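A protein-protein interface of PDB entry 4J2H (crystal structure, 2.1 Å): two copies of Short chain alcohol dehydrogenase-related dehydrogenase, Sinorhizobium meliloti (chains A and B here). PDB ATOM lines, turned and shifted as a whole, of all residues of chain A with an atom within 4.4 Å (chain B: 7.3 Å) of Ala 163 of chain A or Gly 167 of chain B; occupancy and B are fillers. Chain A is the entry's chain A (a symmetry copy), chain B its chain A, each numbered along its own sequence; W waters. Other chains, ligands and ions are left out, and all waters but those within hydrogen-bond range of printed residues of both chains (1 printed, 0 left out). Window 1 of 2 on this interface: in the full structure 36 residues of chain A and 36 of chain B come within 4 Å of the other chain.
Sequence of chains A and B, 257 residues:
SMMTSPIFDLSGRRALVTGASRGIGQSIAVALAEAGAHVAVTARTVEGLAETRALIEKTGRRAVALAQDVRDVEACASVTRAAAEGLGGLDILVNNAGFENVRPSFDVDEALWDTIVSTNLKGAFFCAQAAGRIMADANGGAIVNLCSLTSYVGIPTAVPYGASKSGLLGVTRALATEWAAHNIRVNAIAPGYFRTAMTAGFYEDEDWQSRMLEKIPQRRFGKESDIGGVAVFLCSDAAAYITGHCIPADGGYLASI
The side-chain hydroxyl (OG) of Ser 166 of chain B sits at hydrogen-bond distance from the backbone carbonyl oxygen (O) of Thr 150 of chain B (2.9 Å).
OG of Ser 166 of chain B lies close to O of Gly 162 of chain B.
The side-chain hydroxyl (OG) of Ser 166 of chain A lies close to the backbone carbonyl oxygen (O) of Gly 162 of chain A.
Trp 113 of chain A touches Leu 121 of chain B (CZ2 to CG, 3.7 Å).
Trp 113 of chain A touches Phe 125 of chain B (CZ3 to CG, 3.6 Å).
CG1 of Val 159 of chain A touches CE1 of Phe 125 of chain B (3.4 Å).
CB of Ala 174 of chain B touches CG2 of Val 159 of chain A (3.5 Å).
O of Ala 163 of chain A touches CA of Gly 167 of chain B, 3.3 Å away.
Val 171 of chain B touches Ala 163 of chain A.
Ser 166 of chain B touches Ser 166 of chain A.
Gly 170 of chain B touches Ser 166 of chain A (CA to OG, 3.4 Å).
Gly 167 of chain A touches Ala 163 of chain B.
Gly 167 of chain A touches Gly 167 of chain B.
No residue of chain B comes within 4 Å of Gly 162 of chain A.
Ala 163 of chain A touches just these residues of chain B: Gly 167 (3.3 Å) and Val 171 (3.5 Å).
Printed residues of chain A within 4 Å of Phe 125 of chain B: Trp 113 (3.6 Å) and Val 159 (3.4 Å).
Printed residues of chain A within 4 Å of Ala 163 of chain B: Gly 167.
Gly 167 of chain B touches just these residues of chain A: Ala 163 (3.3 Å) and Gly 167 (3.6 Å).
Leu 169 of chain B touches none of the printed residues of chain A.
Printed residues of chain A within 4 Å of Gly 170 of chain B: Ser 166 (3.4 Å).
Thr 172 of chain B touches none of the printed residues of chain A.
The nearest residue of chain B that does not touch Ala 163 of chain A is Leu 121 of chain B (4.2 Å).
Of the 10 printed residues of chain A, 5 touch a printed residue of chain B.
Ala 163 of chain A touches Gly 167 of chain B, and with the chains exchanged Gly 167 of chain A touches Ala 163 of chain B.
Ser 166 of chain B touches its own counterpart, Ser 166 of chain A.
Gly 167 of chain B touches its own counterpart, Gly 167 of chain A.
Positions printed for both chains: 161, 162, 163, 164, 165, 166 and 167.
Of the 10 pairs that touch across the chains among the printed residues, 4 have their exchanged pair printed and touching as well.
Water W1 bridges OG of Ser 166 of chain A (3.0 Å) and NH1 of Arg 173 of chain B (3.1 Å).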
ATOM      1  N   TRP A 113       9.517  27.119   5.241  1.00  0.00           N
ATOM      2  CA  TRP A 113      10.966  27.054   5.133  1.00  0.00           C
ATOM      3  C   TRP A 113      11.502  25.933   6.006  1.00  0.00           C
ATOM      4  O   TRP A 113      12.263  25.093   5.545  1.00  0.00           O
ATOM      5  CB  TRP A 113      11.637  28.379   5.534  1.00  0.00           C
ATOM      6  CG  TRP A 113      13.129  28.209   5.614  1.00  0.00           C
ATOM      7  CD1 TRP A 113      13.838  27.702   6.669  1.00  0.00           C
ATOM      8  CD2 TRP A 113      14.084  28.503   4.591  1.00  0.00           C
ATOM      9  NE1 TRP A 113      15.175  27.648   6.359  1.00  0.00           N
ATOM     10  CE2 TRP A 113      15.360  28.135   5.091  1.00  0.00           C
ATOM     11  CE3 TRP A 113      13.989  29.021   3.293  1.00  0.00           C
ATOM     12  CZ2 TRP A 113      16.539  28.282   4.340  1.00  0.00           C
ATOM     13  CZ3 TRP A 113      15.159  29.160   2.543  1.00  0.00           C
ATOM     14  CH2 TRP A 113      16.421  28.794   3.072  1.00  0.00           C
ATOM     15  N   VAL A 159      12.460  27.593  -4.061  1.00  0.00           N
ATOM     16  CA  VAL A 159      13.665  28.187  -3.499  1.00  0.00           C
ATOM     17  C   VAL A 159      14.165  27.455  -2.229  1.00  0.00           C
ATOM     18  O   VAL A 159      15.299  26.992  -2.212  1.00  0.00           O
ATOM     19  CB  VAL A 159      13.534  29.716  -3.347  1.00  0.00           C
ATOM     20  CG1 VAL A 159      14.707  30.293  -2.560  1.00  0.00           C
ATOM     21  CG2 VAL A 159      13.497  30.367  -4.736  1.00  0.00           C
ATOM     22  N   PRO A 160      13.319  27.321  -1.189  1.00  0.00           N
ATOM     23  CA  PRO A 160      13.699  26.505  -0.029  1.00  0.00           C
ATOM     24  C   PRO A 160      14.113  25.104  -0.435  1.00  0.00           C
ATOM     25  O   PRO A 160      15.153  24.598   0.054  1.00  0.00           O
ATOM     26  CB  PRO A 160      12.434  26.472   0.822  1.00  0.00           C
ATOM     27  CG  PRO A 160      11.651  27.666   0.398  1.00  0.00           C
ATOM     28  CD  PRO A 160      11.967  27.881  -1.050  1.00  0.00           C
ATOM     29  N   TYR A 161      13.374  24.478  -1.363  1.00  0.00           N
ATOM     30  CA  TYR A 161      13.763  23.116  -1.784  1.00  0.00           C
ATOM     31  C   TYR A 161      15.169  23.113  -2.397  1.00  0.00           C
ATOM     32  O   TYR A 161      15.972  22.228  -2.131  1.00  0.00           O
ATOM     33  CB  TYR A 161      12.767  22.521  -2.768  1.00  0.00           C
ATOM     34  CG  TYR A 161      13.093  21.099  -3.219  1.00  0.00           C
ATOM     35  CD1 TYR A 161      12.702  19.990  -2.461  1.00  0.00           C
ATOM     36  CD2 TYR A 161      13.740  20.862  -4.414  1.00  0.00           C
ATOM     37  CE1 TYR A 161      12.986  18.686  -2.879  1.00  0.00           C
ATOM     38  CE2 TYR A 161      14.026  19.571  -4.839  1.00  0.00           C
ATOM     39  CZ  TYR A 161      13.648  18.490  -4.069  1.00  0.00           C
ATOM     40  OH  TYR A 161      13.920  17.226  -4.516  1.00  0.00           O
ATOM     41  N   GLY A 162      15.440  24.091  -3.261  1.00  0.00           N
ATOM     42  CA  GLY A 162      16.706  24.154  -3.956  1.00  0.00           C
ATOM     43  C   GLY A 162      17.845  24.463  -2.992  1.00  0.00           C
ATOM     44  O   GLY A 162      18.926  23.935  -3.144  1.00  0.00           O
ATOM     45  N   ALA A 163      17.584  25.324  -2.010  1.00  0.00           N
ATOM     46  CA  ALA A 163      18.531  25.578  -0.931  1.00  0.00           C
ATOM     47  C   ALA A 163      18.905  24.289  -0.231  1.00  0.00           C
ATOM     48  O   ALA A 163      20.074  24.066   0.021  1.00  0.00           O
ATOM     49  CB  ALA A 163      17.963  26.563   0.072  1.00  0.00           C
ATOM     50  N   SER A 164      17.897  23.468   0.071  1.00  0.00           N
ATOM     51  CA  SER A 164      18.051  22.169   0.721  1.00  0.00           C
ATOM     52  C   SER A 164      18.951  21.233  -0.005  1.00  0.00           C
ATOM     53  O   SER A 164      19.799  20.595   0.609  1.00  0.00           O
ATOM     54  CB  SER A 164      16.712  21.433   0.815  1.00  0.00           C
ATOM     55  OG  SER A 164      15.913  22.066   1.746  1.00  0.00           O
ATOM     56  N   LYS A 165      18.684  21.072  -1.302  1.00  0.00           N
ATOM     57  CA  LYS A 165      19.385  20.096  -2.105  1.00  0.00           C
ATOM     58  C   LYS A 165      20.785  20.582  -2.561  1.00  0.00           C
ATOM     59  O   LYS A 165      21.689  19.780  -2.780  1.00  0.00           O
ATOM     60  CB  LYS A 165      18.517  19.688  -3.305  1.00  0.00           C
ATOM     61  CG  LYS A 165      17.194  19.015  -2.924  1.00  0.00           C
ATOM     62  CD  LYS A 165      17.431  17.726  -2.177  1.00  0.00           C
ATOM     63  CE  LYS A 165      16.145  16.993  -1.839  1.00  0.00           C
ATOM     64  NZ  LYS A 165      16.445  15.584  -1.484  1.00  0.00           N
ATOM     65  N   SER A 166      20.928  21.890  -2.712  1.00  0.00           N
ATOM     66  CA  SER A 166      22.206  22.519  -2.989  1.00  0.00           C
ATOM     67  C   SER A 166      23.097  22.416  -1.744  1.00  0.00           C
ATOM     68  O   SER A 166      24.271  22.095  -1.843  1.00  0.00           O
ATOM     69  CB  SER A 166      21.968  23.975  -3.398  1.00  0.00           C
ATOM     70  OG  SER A 166      21.665  24.047  -4.790  1.00  0.00           O
ATOM     71  N   GLY A 167      22.501  22.679  -0.586  1.00  0.00           N
ATOM     72  CA  GLY A 167      23.153  22.469   0.689  1.00  0.00           C
ATOM     73  C   GLY A 167      23.606  21.039   0.887  1.00  0.00           C
ATOM     74  O   GLY A 167      24.720  20.798   1.358  1.00  0.00           O
ATOM     75  N   ASN B 120      23.255  31.964   8.351  1.00  0.00           N
ATOM     76  CA  ASN B 120      23.887  32.037   7.031  1.00  0.00           C
ATOM     77  C   ASN B 120      22.966  31.821   5.832  1.00  0.00           C
ATOM     78  O   ASN B 120      23.257  32.329   4.755  1.00  0.00           O
ATOM     79  CB  ASN B 120      25.031  31.027   6.922  1.00  0.00           C
ATOM     80  CG  ASN B 120      26.163  31.313   7.887  1.00  0.00           C
ATOM     81  OD1 ASN B 120      26.109  32.260   8.637  1.00  0.00           O
ATOM     82  ND2 ASN B 120      27.169  30.486   7.878  1.00  0.00           N
ATOM     83  N   LEU B 121      21.893  31.051   6.000  1.00  0.00           N
ATOM     84  CA  LEU B 121      21.077  30.642   4.848  1.00  0.00           C
ATOM     85  C   LEU B 121      19.659  31.172   4.974  1.00  0.00           C
ATOM     86  O   LEU B 121      19.197  31.869   4.108  1.00  0.00           O
ATOM     87  CB  LEU B 121      21.044  29.118   4.704  1.00  0.00           C
ATOM     88  CG  LEU B 121      20.190  28.505   3.586  1.00  0.00           C
ATOM     89  CD1 LEU B 121      20.508  29.142   2.240  1.00  0.00           C
ATOM     90  CD2 LEU B 121      20.399  27.003   3.517  1.00  0.00           C
ATOM     91  N   PHE B 125      17.645  34.340   3.044  1.00  0.00           N
ATOM     92  CA  PHE B 125      16.418  34.136   2.295  1.00  0.00           C
ATOM     93  C   PHE B 125      15.392  35.166   2.720  1.00  0.00           C
ATOM     94  O   PHE B 125      14.818  35.852   1.881  1.00  0.00           O
ATOM     95  CB  PHE B 125      15.821  32.737   2.461  1.00  0.00           C
ATOM     96  CG  PHE B 125      14.477  32.585   1.778  1.00  0.00           C
ATOM     97  CD1 PHE B 125      14.400  32.411   0.399  1.00  0.00           C
ATOM     98  CD2 PHE B 125      13.298  32.662   2.498  1.00  0.00           C
ATOM     99  CE1 PHE B 125      13.169  32.299  -0.242  1.00  0.00           C
ATOM    100  CE2 PHE B 125      12.063  32.553   1.866  1.00  0.00           C
ATOM    101  CZ  PHE B 125      11.999  32.375   0.489  1.00  0.00           C
ATOM    102  N   CYS B 147      28.700  34.042  -0.628  1.00  0.00           N
ATOM    103  CA  CYS B 147      28.901  32.614  -0.573  1.00  0.00           C
ATOM    104  C   CYS B 147      30.360  32.397  -0.109  1.00  0.00           C
ATOM    105  O   CYS B 147      30.863  33.199   0.633  1.00  0.00           O
ATOM    106  CB  CYS B 147      28.594  31.984  -1.920  1.00  0.00           C
ATOM    107  SG  CYS B 147      26.808  32.006  -2.290  1.00  0.00           S
ATOM    108  N   THR B 150      33.331  27.092   0.183  1.00  0.00           N
ATOM    109  CA  THR B 150      32.552  25.936   0.593  1.00  0.00           C
ATOM    110  C   THR B 150      31.248  25.743  -0.226  1.00  0.00           C
ATOM    111  O   THR B 150      30.547  24.733  -0.022  1.00  0.00           O
ATOM    112  CB  THR B 150      32.199  25.986   2.078  1.00  0.00           C
ATOM    113  OG1 THR B 150      31.363  27.110   2.335  1.00  0.00           O
ATOM    114  CG2 THR B 150      33.460  26.086   2.956  1.00  0.00           C
ATOM    115  N   SER B 151      30.953  26.687  -1.128  1.00  0.00           N
ATOM    116  CA  SER B 151      29.884  26.514  -2.147  1.00  0.00           C
ATOM    117  C   SER B 151      30.357  25.638  -3.302  1.00  0.00           C
ATOM    118  O   SER B 151      29.543  25.168  -4.091  1.00  0.00           O
ATOM    119  CB  SER B 151      29.419  27.876  -2.677  1.00  0.00           C
ATOM    120  OG  SER B 151      29.039  28.719  -1.592  1.00  0.00           O
ATOM    121  N   TYR B 161      28.421  24.887   8.041  1.00  0.00           N
ATOM    122  CA  TYR B 161      28.744  26.139   7.328  1.00  0.00           C
ATOM    123  C   TYR B 161      28.676  25.937   5.808  1.00  0.00           C
ATOM    124  O   TYR B 161      28.162  26.777   5.082  1.00  0.00           O
ATOM    125  CB  TYR B 161      30.112  26.677   7.719  1.00  0.00           C
ATOM    126  CG  TYR B 161      30.495  27.990   7.040  1.00  0.00           C
ATOM    127  CD1 TYR B 161      30.084  29.222   7.561  1.00  0.00           C
ATOM    128  CD2 TYR B 161      31.301  28.005   5.921  1.00  0.00           C
ATOM    129  CE1 TYR B 161      30.445  30.427   6.950  1.00  0.00           C
ATOM    130  CE2 TYR B 161      31.667  29.196   5.307  1.00  0.00           C
ATOM    131  CZ  TYR B 161      31.236  30.401   5.825  1.00  0.00           C
ATOM    132  OH  TYR B 161      31.626  31.563   5.217  1.00  0.00           O
ATOM    133  N   GLY B 162      29.246  24.830   5.333  1.00  0.00           N
ATOM    134  CA  GLY B 162      29.307  24.564   3.914  1.00  0.00           C
ATOM    135  C   GLY B 162      27.919  24.293   3.347  1.00  0.00           C
ATOM    136  O   GLY B 162      27.626  24.700   2.243  1.00  0.00           O
ATOM    137  N   ALA B 163      27.081  23.600   4.116  1.00  0.00           N
ATOM    138  CA  ALA B 163      25.678  23.416   3.763  1.00  0.00           C
ATOM    139  C   ALA B 163      24.999  24.752   3.549  1.00  0.00           C
ATOM    140  O   ALA B 163      24.280  24.906   2.580  1.00  0.00           O
ATOM    141  CB  ALA B 163      24.945  22.631   4.833  1.00  0.00           C
ATOM    142  N   SER B 164      25.241  25.690   4.467  1.00  0.00           N
ATOM    143  CA  SER B 164      24.704  27.048   4.427  1.00  0.00           C
ATOM    144  C   SER B 164      25.040  27.795   3.185  1.00  0.00           C
ATOM    145  O   SER B 164      24.173  28.435   2.600  1.00  0.00           O
ATOM    146  CB  SER B 164      25.270  27.902   5.564  1.00  0.00           C
ATOM    147  OG  SER B 164      24.733  27.474   6.762  1.00  0.00           O
ATOM    148  N   LYS B 165      26.331  27.799   2.851  1.00  0.00           N
ATOM    149  CA  LYS B 165      26.826  28.591   1.748  1.00  0.00           C
ATOM    150  C   LYS B 165      26.578  27.929   0.368  1.00  0.00           C
ATOM    151  O   LYS B 165      26.446  28.612  -0.644  1.00  0.00           O
ATOM    152  CB  LYS B 165      28.315  28.904   1.958  1.00  0.00           C
ATOM    153  CG  LYS B 165      28.612  29.734   3.212  1.00  0.00           C
ATOM    154  CD  LYS B 165      27.951  31.088   3.140  1.00  0.00           C
ATOM    155  CE  LYS B 165      28.276  31.969   4.334  1.00  0.00           C
ATOM    156  NZ  LYS B 165      27.947  33.382   4.024  1.00  0.00           N
ATOM    157  N   SER B 166      26.537  26.605   0.355  1.00  0.00           N
ATOM    158  CA  SER B 166      26.171  25.836  -0.819  1.00  0.00           C
ATOM    159  C   SER B 166      24.675  26.032  -1.101  1.00  0.00           C
ATOM    160  O   SER B 166      24.277  26.235  -2.237  1.00  0.00           O
ATOM    161  CB  SER B 166      26.516  24.364  -0.581  1.00  0.00           C
ATOM    162  OG  SER B 166      27.888  24.128  -0.892  1.00  0.00           O
ATOM    163  N   GLY B 167      23.878  25.983  -0.040  1.00  0.00           N
ATOM    164  CA  GLY B 167      22.470  26.309  -0.109  1.00  0.00           C
ATOM    165  C   GLY B 167      22.217  27.708  -0.627  1.00  0.00           C
ATOM    166  O   GLY B 167      21.328  27.915  -1.456  1.00  0.00           O
ATOM    167  N   LEU B 168      23.005  28.673  -0.162  1.00  0.00           N
ATOM    168  CA  LEU B 168      22.817  30.054  -0.591  1.00  0.00           C
ATOM    169  C   LEU B 168      23.126  30.253  -2.094  1.00  0.00           C
ATOM    170  O   LEU B 168      22.531  31.106  -2.774  1.00  0.00           O
ATOM    171  CB  LEU B 168      23.640  30.997   0.286  1.00  0.00           C
ATOM    172  CG  LEU B 168      23.392  32.491   0.115  1.00  0.00           C
ATOM    173  CD1 LEU B 168      21.917  32.813   0.359  1.00  0.00           C
ATOM    174  CD2 LEU B 168      24.294  33.255   1.075  1.00  0.00           C
ATOM    175  N   LEU B 169      24.057  29.481  -2.619  1.00  0.00           N
ATOM    176  CA  LEU B 169      24.270  29.486  -4.033  1.00  0.00           C
ATOM    177  C   LEU B 169      23.018  28.930  -4.769  1.00  0.00           C
ATOM    178  O   LEU B 169      22.657  29.435  -5.797  1.00  0.00           O
ATOM    179  CB  LEU B 169      25.477  28.642  -4.408  1.00  0.00           C
ATOM    180  CG  LEU B 169      25.887  28.696  -5.874  1.00  0.00           C
ATOM    181  CD1 LEU B 169      25.902  30.126  -6.410  1.00  0.00           C
ATOM    182  CD2 LEU B 169      27.253  28.045  -6.105  1.00  0.00           C
ATOM    183  N   GLY B 170      22.404  27.870  -4.240  1.00  0.00           N
ATOM    184  CA  GLY B 170      21.152  27.382  -4.798  1.00  0.00           C
ATOM    185  C   GLY B 170      20.072  28.447  -4.736  1.00  0.00           C
ATOM    186  O   GLY B 170      19.268  28.574  -5.663  1.00  0.00           O
ATOM    187  N   VAL B 171      20.057  29.219  -3.653  1.00  0.00           N
ATOM    188  CA  VAL B 171      19.093  30.286  -3.459  1.00  0.00           C
ATOM    189  C   VAL B 171      19.304  31.387  -4.490  1.00  0.00           C
ATOM    190  O   VAL B 171      18.337  31.931  -5.046  1.00  0.00           O
ATOM    191  CB  VAL B 171      19.164  30.859  -2.038  1.00  0.00           C
ATOM    192  CG1 VAL B 171      18.362  32.146  -1.899  1.00  0.00           C
ATOM    193  CG2 VAL B 171      18.659  29.832  -1.040  1.00  0.00           C
ATOM    194  N   THR B 172      20.567  31.711  -4.726  1.00  0.00           N
ATOM    195  CA  THR B 172      20.955  32.686  -5.715  1.00  0.00           C
ATOM    196  C   THR B 172      20.429  32.305  -7.118  1.00  0.00           C
ATOM    197  O   THR B 172      19.847  33.140  -7.814  1.00  0.00           O
ATOM    198  CB  THR B 172      22.507  32.863  -5.700  1.00  0.00           C
ATOM    199  OG1 THR B 172      22.928  33.331  -4.396  1.00  0.00           O
ATOM    200  CG2 THR B 172      22.958  33.799  -6.746  1.00  0.00           C
ATOM    201  N   ARG B 173      20.584  31.049  -7.507  1.00  0.00           N
ATOM    202  CA  ARG B 173      20.133  30.607  -8.813  1.00  0.00           C
ATOM    203  C   ARG B 173      18.596  30.587  -8.977  1.00  0.00           C
ATOM    204  O   ARG B 173      18.089  31.043  -9.991  1.00  0.00           O
ATOM    205  CB  ARG B 173      20.701  29.242  -9.130  1.00  0.00           C
ATOM    206  CG  ARG B 173      22.221  29.245  -9.361  1.00  0.00           C
ATOM    207  CD  ARG B 173      22.707  27.835  -9.354  1.00  0.00           C
ATOM    208  NE  ARG B 173      24.144  27.725  -9.657  1.00  0.00           N
ATOM    209  CZ  ARG B 173      24.908  26.742  -9.180  1.00  0.00           C
ATOM    210  NH1 ARG B 173      24.390  25.807  -8.412  1.00  0.00           N
ATOM    211  NH2 ARG B 173      26.183  26.680  -9.494  1.00  0.00           N
ATOM    212  N   ALA B 174      17.888  30.056  -7.990  1.00  0.00           N
ATOM    213  CA  ALA B 174      16.425  29.966  -8.028  1.00  0.00           C
ATOM    214  C   ALA B 174      15.742  31.330  -7.940  1.00  0.00           C
ATOM    215  O   ALA B 174      14.831  31.610  -8.733  1.00  0.00           O
ATOM    216  CB  ALA B 174      15.927  29.034  -6.949  1.00  0.00           C
HETATM  217  O   HOH W   1      21.485  25.329  -7.442  1.00  0.00           O
